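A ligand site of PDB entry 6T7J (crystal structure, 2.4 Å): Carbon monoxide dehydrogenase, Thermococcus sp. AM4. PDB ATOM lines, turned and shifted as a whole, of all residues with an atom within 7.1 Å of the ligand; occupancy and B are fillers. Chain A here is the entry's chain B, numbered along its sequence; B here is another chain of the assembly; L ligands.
FE1 of the ligand is bound by SG of Cys 77 (2.3 Å). The side-chain sulfur of Cys 63 is bound to an iron atom (FE3) of the ligand, at 2.7 Å. SG of Cys 55 binds FE2 of the ligand (2.4 Å). S3 of the ligand sits close to NH2 of Arg 87 (3.3 Å). SG of Cys 58 binds FE4 of the ligand (2.5 Å). N of Cys 77 sits close to S2 of the ligand (3.2 Å). The backbone NH (N) of Asn 57 lies close to a sulfur (S1) of the ligand, at 3.8 Å.
SG of Cys 63 sits close to N of Val 76, 3.2 Å away. The side-chain sulfur (SG) of Cys 77 sits close to the backbone NH (N) of Ala 79 (3.2 Å). O of Met 60 sits at hydrogen-bond distance from NE2 of Gln 45 of chain B, 2.9 Å away. N of Cys 55 sits at hydrogen-bond distance from O of Cys 63 (3.0 Å). The side-chain sulfur of Cys 58 lies close to the backbone NH of Met 60. ND2 of Asn 57 is in hydrogen-bond range of O of Thr 204, 3.0 Å away. SG of Cys 55 sits close to NH2 of Arg 87 (3.5 Å). The side-chain amide oxygen of Gln 45 of chain B lies close to the backbone carbonyl oxygen of Gly 61 (3.5 Å).
Residues that only touch the ligand: Gly 61 (3.6 Å), Met 60 (3.7 Å), Val 76 (3.7 Å), Ile 206 (3.8 Å), Gly 75 (3.95 Å) and Ile 84 (3.96 Å). Hydrophobic or aromatic side chains within 4 Å of the ligand: Met 60, Val 76, Ile 84 and Ile 206. Of the 29 residues printed, 12 come within 4 Å of the ligand. The nearest printed residue that does not touch the ligand is Ala 79 (4.03 Å).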
ATOM      1  N   CYS A  54     -12.856   5.846  25.177  1.00  0.00           N
ATOM      2  CA  CYS A  54     -14.273   5.901  25.483  1.00  0.00           C
ATOM      3  C   CYS A  54     -14.985   4.786  24.729  1.00  0.00           C
ATOM      4  O   CYS A  54     -14.841   4.670  23.513  1.00  0.00           O
ATOM      5  CB  CYS A  54     -14.886   7.263  25.127  1.00  0.00           C
ATOM      6  SG  CYS A  54     -16.686   7.240  24.978  1.00  0.00           S
ATOM      7  N   CYS A  55     -15.746   3.980  25.457  1.00  0.00           N
ATOM      8  CA  CYS A  55     -16.341   2.764  24.917  1.00  0.00           C
ATOM      9  C   CYS A  55     -17.859   2.784  25.065  1.00  0.00           C
ATOM     10  O   CYS A  55     -18.388   3.205  26.099  1.00  0.00           O
ATOM     11  CB  CYS A  55     -15.764   1.525  25.608  1.00  0.00           C
ATOM     12  SG  CYS A  55     -16.522  -0.030  25.145  1.00  0.00           S
ATOM     13  N   ARG A  56     -18.541   2.325  24.044  1.00  0.00           N
ATOM     14  CA  ARG A  56     -19.959   2.296  24.013  1.00  0.00           C
ATOM     15  C   ARG A  56     -20.380   0.935  23.555  1.00  0.00           C
ATOM     16  O   ARG A  56     -21.357   0.776  22.883  1.00  0.00           O
ATOM     17  CB  ARG A  56     -20.457   3.360  23.043  1.00  0.00           C
ATOM     18  CG  ARG A  56     -20.078   4.763  23.440  1.00  0.00           C
ATOM     19  CD  ARG A  56     -20.685   5.790  22.528  1.00  0.00           C
ATOM     20  NE  ARG A  56     -20.647   5.325  21.170  1.00  0.00           N
ATOM     21  CZ  ARG A  56     -20.174   6.016  20.144  1.00  0.00           C
ATOM     22  NH1 ARG A  56     -19.694   7.229  20.338  1.00  0.00           N
ATOM     23  NH2 ARG A  56     -20.174   5.498  18.952  1.00  0.00           N
ATOM     24  N   ASN A  57     -19.653  -0.074  23.958  1.00  0.00           N
ATOM     25  CA  ASN A  57     -19.945  -1.429  23.522  1.00  0.00           C
ATOM     26  C   ASN A  57     -21.070  -2.130  24.250  1.00  0.00           C
ATOM     27  O   ASN A  57     -21.466  -3.205  23.869  1.00  0.00           O
ATOM     28  CB  ASN A  57     -18.688  -2.266  23.477  1.00  0.00           C
ATOM     29  CG  ASN A  57     -17.769  -1.852  22.380  1.00  0.00           C
ATOM     30  OD1 ASN A  57     -17.967  -0.852  21.759  1.00  0.00           O
ATOM     31  ND2 ASN A  57     -16.743  -2.600  22.161  1.00  0.00           N
ATOM     32  N   CYS A  58     -21.596  -1.521  25.291  1.00  0.00           N
ATOM     33  CA  CYS A  58     -22.701  -2.112  26.000  1.00  0.00           C
ATOM     34  C   CYS A  58     -23.541  -1.031  26.629  1.00  0.00           C
ATOM     35  O   CYS A  58     -23.156   0.097  26.668  1.00  0.00           O
ATOM     36  CB  CYS A  58     -22.232  -3.154  26.993  1.00  0.00           C
ATOM     37  SG  CYS A  58     -21.793  -2.624  28.627  1.00  0.00           S
ATOM     38  N   ALA A  59     -24.721  -1.402  27.089  1.00  0.00           N
ATOM     39  CA  ALA A  59     -25.640  -0.470  27.691  1.00  0.00           C
ATOM     40  C   ALA A  59     -25.267   0.005  29.073  1.00  0.00           C
ATOM     41  O   ALA A  59     -25.926   0.857  29.605  1.00  0.00           O
ATOM     42  CB  ALA A  59     -27.046  -0.992  27.654  1.00  0.00           C
ATOM     43  N   MET A  60     -24.263  -0.591  29.695  1.00  0.00           N
ATOM     44  CA  MET A  60     -23.785  -0.052  30.963  1.00  0.00           C
ATOM     45  C   MET A  60     -22.912   1.175  30.768  1.00  0.00           C
ATOM     46  O   MET A  60     -22.612   1.865  31.751  1.00  0.00           O
ATOM     47  CB  MET A  60     -23.000  -1.124  31.721  1.00  0.00           C
ATOM     48  CG  MET A  60     -23.704  -2.463  31.826  1.00  0.00           C
ATOM     49  SD  MET A  60     -22.954  -3.519  33.076  1.00  0.00           S
ATOM     50  CE  MET A  60     -21.365  -3.868  32.325  1.00  0.00           C
ATOM     51  N   GLY A  61     -22.494   1.464  29.534  1.00  0.00           N
ATOM     52  CA  GLY A  61     -21.766   2.662  29.227  1.00  0.00           C
ATOM     53  C   GLY A  61     -22.698   3.811  28.892  1.00  0.00           C
ATOM     54  O   GLY A  61     -23.891   3.766  29.195  1.00  0.00           O
ATOM     55  N   PRO A  62     -22.167   4.865  28.254  1.00  0.00           N
ATOM     56  CA  PRO A  62     -20.783   5.006  27.786  1.00  0.00           C
ATOM     57  C   PRO A  62     -19.794   5.154  28.951  1.00  0.00           C
ATOM     58  O   PRO A  62     -20.152   5.704  29.985  1.00  0.00           O
ATOM     59  CB  PRO A  62     -20.811   6.288  26.940  1.00  0.00           C
ATOM     60  CG  PRO A  62     -22.270   6.624  26.750  1.00  0.00           C
ATOM     61  CD  PRO A  62     -22.966   6.062  27.933  1.00  0.00           C
ATOM     62  N   CYS A  63     -18.583   4.645  28.783  1.00  0.00           N
ATOM     63  CA  CYS A  63     -17.558   4.729  29.811  1.00  0.00           C
ATOM     64  C   CYS A  63     -16.343   5.479  29.273  1.00  0.00           C
ATOM     65  O   CYS A  63     -15.885   5.229  28.152  1.00  0.00           O
ATOM     66  CB  CYS A  63     -17.108   3.350  30.304  1.00  0.00           C
ATOM     67  SG  CYS A  63     -18.177   2.458  31.433  1.00  0.00           S
ATOM     68  N   ARG A  64     -15.824   6.379  30.100  1.00  0.00           N
ATOM     69  CA  ARG A  64     -14.619   7.146  29.839  1.00  0.00           C
ATOM     70  C   ARG A  64     -13.497   6.670  30.742  1.00  0.00           C
ATOM     71  O   ARG A  64     -13.708   6.419  31.931  1.00  0.00           O
ATOM     72  CB  ARG A  64     -14.829   8.632  30.119  1.00  0.00           C
ATOM     73  CG  ARG A  64     -15.660   9.404  29.127  1.00  0.00           C
ATOM     74  CD  ARG A  64     -16.357  10.512  29.890  1.00  0.00           C
ATOM     75  NE  ARG A  64     -16.790  11.619  29.031  1.00  0.00           N
ATOM     76  CZ  ARG A  64     -17.529  12.640  29.461  1.00  0.00           C
ATOM     77  NH1 ARG A  64     -17.914  12.687  30.734  1.00  0.00           N
ATOM     78  NH2 ARG A  64     -17.885  13.599  28.621  1.00  0.00           N
ATOM     79  N   ILE A  65     -12.287   6.567  30.194  1.00  0.00           N
ATOM     80  CA  ILE A  65     -11.099   6.319  30.993  1.00  0.00           C
ATOM     81  C   ILE A  65     -10.267   7.594  30.995  1.00  0.00           C
ATOM     82  O   ILE A  65      -9.915   8.114  29.922  1.00  0.00           O
ATOM     83  CB  ILE A  65     -10.285   5.130  30.470  1.00  0.00           C
ATOM     84  CG1 ILE A  65     -11.152   3.877  30.418  1.00  0.00           C
ATOM     85  CG2 ILE A  65      -9.063   4.902  31.360  1.00  0.00           C
ATOM     86  CD1 ILE A  65     -11.978   3.650  31.666  1.00  0.00           C
ATOM     87  N   LYS A  74     -11.208   2.653  35.077  1.00  0.00           N
ATOM     88  CA  LYS A  74     -11.781   1.439  34.517  1.00  0.00           C
ATOM     89  C   LYS A  74     -13.253   1.643  34.236  1.00  0.00           C
ATOM     90  O   LYS A  74     -13.946   2.367  34.956  1.00  0.00           O
ATOM     91  CB  LYS A  74     -11.583   0.248  35.470  1.00  0.00           C
ATOM     92  CG  LYS A  74     -10.166  -0.290  35.480  1.00  0.00           C
ATOM     93  CD  LYS A  74      -9.965  -1.322  36.555  1.00  0.00           C
ATOM     94  CE  LYS A  74      -9.085  -2.422  36.041  1.00  0.00           C
ATOM     95  NZ  LYS A  74      -9.527  -3.657  36.639  1.00  0.00           N
ATOM     96  N   GLY A  75     -13.733   1.005  33.167  1.00  0.00           N
ATOM     97  CA  GLY A  75     -15.141   1.060  32.818  1.00  0.00           C
ATOM     98  C   GLY A  75     -15.991   0.232  33.775  1.00  0.00           C
ATOM     99  O   GLY A  75     -15.498  -0.430  34.689  1.00  0.00           O
ATOM    100  N   VAL A  76     -17.307   0.287  33.546  1.00  0.00           N
ATOM    101  CA  VAL A  76     -18.243  -0.436  34.406  1.00  0.00           C
ATOM    102  C   VAL A  76     -17.925  -1.931  34.402  1.00  0.00           C
ATOM    103  O   VAL A  76     -17.974  -2.593  35.441  1.00  0.00           O
ATOM    104  CB  VAL A  76     -19.697  -0.153  33.974  1.00  0.00           C
ATOM    105  CG1 VAL A  76     -20.667  -0.957  34.811  1.00  0.00           C
ATOM    106  CG2 VAL A  76     -20.014   1.324  34.076  1.00  0.00           C
ATOM    107  N   CYS A  77     -17.585  -2.469  33.227  1.00  0.00           N
ATOM    108  CA  CYS A  77     -17.209  -3.872  33.086  1.00  0.00           C
ATOM    109  C   CYS A  77     -15.851  -4.195  33.685  1.00  0.00           C
ATOM    110  O   CYS A  77     -15.533  -5.373  33.872  1.00  0.00           O
ATOM    111  CB  CYS A  77     -17.195  -4.250  31.601  1.00  0.00           C
ATOM    112  SG  CYS A  77     -15.797  -3.570  30.698  1.00  0.00           S
ATOM    113  N   GLY A  78     -15.042  -3.186  33.989  1.00  0.00           N
ATOM    114  CA  GLY A  78     -13.672  -3.390  34.415  1.00  0.00           C
ATOM    115  C   GLY A  78     -12.632  -3.223  33.336  1.00  0.00           C
ATOM    116  O   GLY A  78     -11.455  -3.474  33.608  1.00  0.00           O
ATOM    117  N   ALA A  79     -13.021  -2.804  32.136  1.00  0.00           N
ATOM    118  CA  ALA A  79     -12.062  -2.669  31.037  1.00  0.00           C
ATOM    119  C   ALA A  79     -11.153  -1.475  31.261  1.00  0.00           C
ATOM    120  O   ALA A  79     -11.616  -0.355  31.466  1.00  0.00           O
ATOM    121  CB  ALA A  79     -12.795  -2.525  29.702  1.00  0.00           C
ATOM    122  N   GLY A  80      -9.842  -1.732  31.218  1.00  0.00           N
ATOM    123  CA  GLY A  80      -8.869  -0.663  31.268  1.00  0.00           C
ATOM    124  C   GLY A  80      -8.772   0.071  29.943  1.00  0.00           C
ATOM    125  O   GLY A  80      -9.484  -0.203  28.971  1.00  0.00           O
ATOM    126  N   ILE A  84      -9.952  -0.962  25.900  1.00  0.00           N
ATOM    127  CA  ILE A  84     -10.931  -0.158  25.166  1.00  0.00           C
ATOM    128  C   ILE A  84     -10.328   0.385  23.873  1.00  0.00           C
ATOM    129  O   ILE A  84     -10.955   0.331  22.807  1.00  0.00           O
ATOM    130  CB  ILE A  84     -11.458   0.963  26.081  1.00  0.00           C
ATOM    131  CG1 ILE A  84     -12.312   0.366  27.195  1.00  0.00           C
ATOM    132  CG2 ILE A  84     -12.254   1.974  25.269  1.00  0.00           C
ATOM    133  CD1 ILE A  84     -12.495   1.270  28.396  1.00  0.00           C
ATOM    134  N   ARG A  87      -9.918  -2.512  21.380  1.00  0.00           N
ATOM    135  CA  ARG A  87     -11.198  -2.958  20.839  1.00  0.00           C
ATOM    136  C   ARG A  87     -11.729  -1.983  19.805  1.00  0.00           C
ATOM    137  O   ARG A  87     -12.222  -2.390  18.734  1.00  0.00           O
ATOM    138  CB  ARG A  87     -12.214  -3.156  21.961  1.00  0.00           C
ATOM    139  CG  ARG A  87     -11.972  -4.391  22.818  1.00  0.00           C
ATOM    140  CD  ARG A  87     -13.189  -4.720  23.679  1.00  0.00           C
ATOM    141  NE  ARG A  87     -13.556  -3.631  24.580  1.00  0.00           N
ATOM    142  CZ  ARG A  87     -14.370  -3.768  25.624  1.00  0.00           C
ATOM    143  NH1 ARG A  87     -14.895  -4.953  25.905  1.00  0.00           N
ATOM    144  NH2 ARG A  87     -14.661  -2.725  26.395  1.00  0.00           N
ATOM    145  N   THR A 204     -14.615  -7.865  20.356  1.00  0.00           N
ATOM    146  CA  THR A 204     -14.845  -6.565  20.980  1.00  0.00           C
ATOM    147  C   THR A 204     -16.146  -6.498  21.760  1.00  0.00           C
ATOM    148  O   THR A 204     -16.351  -5.538  22.509  1.00  0.00           O
ATOM    149  CB  THR A 204     -14.841  -5.480  19.907  1.00  0.00           C
ATOM    150  OG1 THR A 204     -15.935  -5.693  19.001  1.00  0.00           O
ATOM    151  CG2 THR A 204     -13.536  -5.498  19.125  1.00  0.00           C
ATOM    152  N   HIS A 205     -17.034  -7.488  21.592  1.00  0.00           N
ATOM    153  CA  HIS A 205     -18.230  -7.573  22.415  1.00  0.00           C
ATOM    154  C   HIS A 205     -17.850  -7.578  23.896  1.00  0.00           C
ATOM    155  O   HIS A 205     -16.755  -8.019  24.271  1.00  0.00           O
ATOM    156  CB  HIS A 205     -19.004  -8.848  22.055  1.00  0.00           C
ATOM    157  CG  HIS A 205     -20.375  -8.934  22.673  1.00  0.00           C
ATOM    158  ND1 HIS A 205     -20.571  -9.263  23.993  1.00  0.00           N
ATOM    159  CD2 HIS A 205     -21.598  -8.748  22.144  1.00  0.00           C
ATOM    160  CE1 HIS A 205     -21.868  -9.271  24.247  1.00  0.00           C
ATOM    161  NE2 HIS A 205     -22.515  -8.962  23.146  1.00  0.00           N
ATOM    162  N   ILE A 206     -18.748  -7.052  24.735  1.00  0.00           N
ATOM    163  CA  ILE A 206     -18.425  -6.941  26.155  1.00  0.00           C
ATOM    164  C   ILE A 206     -18.132  -8.320  26.725  1.00  0.00           C
ATOM    165  O   ILE A 206     -18.850  -9.294  26.456  1.00  0.00           O
ATOM    166  CB  ILE A 206     -19.558  -6.254  26.927  1.00  0.00           C
ATOM    167  CG1 ILE A 206     -19.208  -6.248  28.412  1.00  0.00           C
ATOM    168  CG2 ILE A 206     -20.901  -6.948  26.696  1.00  0.00           C
ATOM    169  CD1 ILE A 206     -20.002  -5.293  29.241  1.00  0.00           C
ATOM    170  N   GLY A 207     -17.039  -8.410  27.473  1.00  0.00           N
ATOM    171  CA  GLY A 207     -16.713  -9.641  28.161  1.00  0.00           C
ATOM    172  C   GLY A 207     -16.200 -10.766  27.290  1.00  0.00           C
ATOM    173  O   GLY A 207     -16.395 -11.935  27.624  1.00  0.00           O
ATOM    174  N   GLN B  42     -18.549   6.434  36.882  1.00  0.00           N
ATOM    175  CA  GLN B  42     -18.770   6.924  35.520  1.00  0.00           C
ATOM    176  C   GLN B  42     -19.752   8.092  35.459  1.00  0.00           C
ATOM    177  O   GLN B  42     -19.793   8.780  34.438  1.00  0.00           O
ATOM    178  CB  GLN B  42     -19.271   5.792  34.623  1.00  0.00           C
ATOM    179  CG  GLN B  42     -18.217   4.757  34.273  1.00  0.00           C
ATOM    180  CD  GLN B  42     -17.074   5.339  33.453  1.00  0.00           C
ATOM    181  OE1 GLN B  42     -17.265   6.282  32.684  1.00  0.00           O
ATOM    182  NE2 GLN B  42     -15.893   4.764  33.614  1.00  0.00           N
ATOM    183  N   GLN B  45     -22.746  10.076  33.057  1.00  0.00           N
ATOM    184  CA  GLN B  45     -22.330   9.520  31.782  1.00  0.00           C
ATOM    185  C   GLN B  45     -22.735  10.457  30.641  1.00  0.00           C
ATOM    186  O   GLN B  45     -23.742  11.169  30.717  1.00  0.00           O
ATOM    187  CB  GLN B  45     -22.943   8.129  31.571  1.00  0.00           C
ATOM    188  CG  GLN B  45     -22.275   7.054  32.409  1.00  0.00           C
ATOM    189  CD  GLN B  45     -22.984   5.723  32.324  1.00  0.00           C
ATOM    190  OE1 GLN B  45     -24.191   5.650  32.120  1.00  0.00           O
ATOM    191  NE2 GLN B  45     -22.224   4.637  32.485  1.00  0.00           N
ATOM    192  N   PRO B 346     -13.833  -8.356  32.715  1.00  0.00           N
ATOM    193  CA  PRO B 346     -12.397  -8.360  33.006  1.00  0.00           C
ATOM    194  C   PRO B 346     -12.097  -8.114  34.478  1.00  0.00           C
ATOM    195  O   PRO B 346     -11.123  -8.651  35.015  1.00  0.00           O
ATOM    196  CB  PRO B 346     -11.850  -7.232  32.117  1.00  0.00           C
ATOM    197  CG  PRO B 346     -12.862  -7.092  31.011  1.00  0.00           C
ATOM    198  CD  PRO B 346     -14.191  -7.412  31.633  1.00  0.00           C
ATOM    199  N   MET B 556     -28.269  -5.328  28.668  1.00  0.00           N
ATOM    200  CA  MET B 556     -27.076  -4.493  28.502  1.00  0.00           C
ATOM    201  C   MET B 556     -26.218  -4.860  27.291  1.00  0.00           C
ATOM    202  O   MET B 556     -25.481  -3.991  26.809  1.00  0.00           O
ATOM    203  CB  MET B 556     -26.199  -4.535  29.754  1.00  0.00           C
ATOM    204  CG  MET B 556     -25.529  -5.888  30.025  1.00  0.00           C
ATOM    205  SD  MET B 556     -23.935  -6.130  29.188  1.00  0.00           S
ATOM    206  CE  MET B 556     -23.750  -7.902  29.344  1.00  0.00           C
HETATM  207 FE1  LIG L   1     -17.222  -2.211  29.507  1.00  0.00          FE
HETATM  208 FE2  LIG L   1     -17.303  -0.616  27.286  1.00  0.00          FE
HETATM  209 FE3  LIG L   1     -18.225   0.388  29.713  1.00  0.00          FE
HETATM  210 FE4  LIG L   1     -19.487  -1.619  28.281  1.00  0.00          FE
HETATM  211  S1  LIG L   1     -19.220   0.587  27.652  1.00  0.00           S
HETATM  212  S2  LIG L   1     -19.132  -1.536  30.574  1.00  0.00           S
HETATM  213  S3  LIG L   1     -17.804  -2.871  27.376  1.00  0.00           S
HETATM  214  S4  LIG L   1     -16.071  -0.235  29.200  1.00  0.00           S
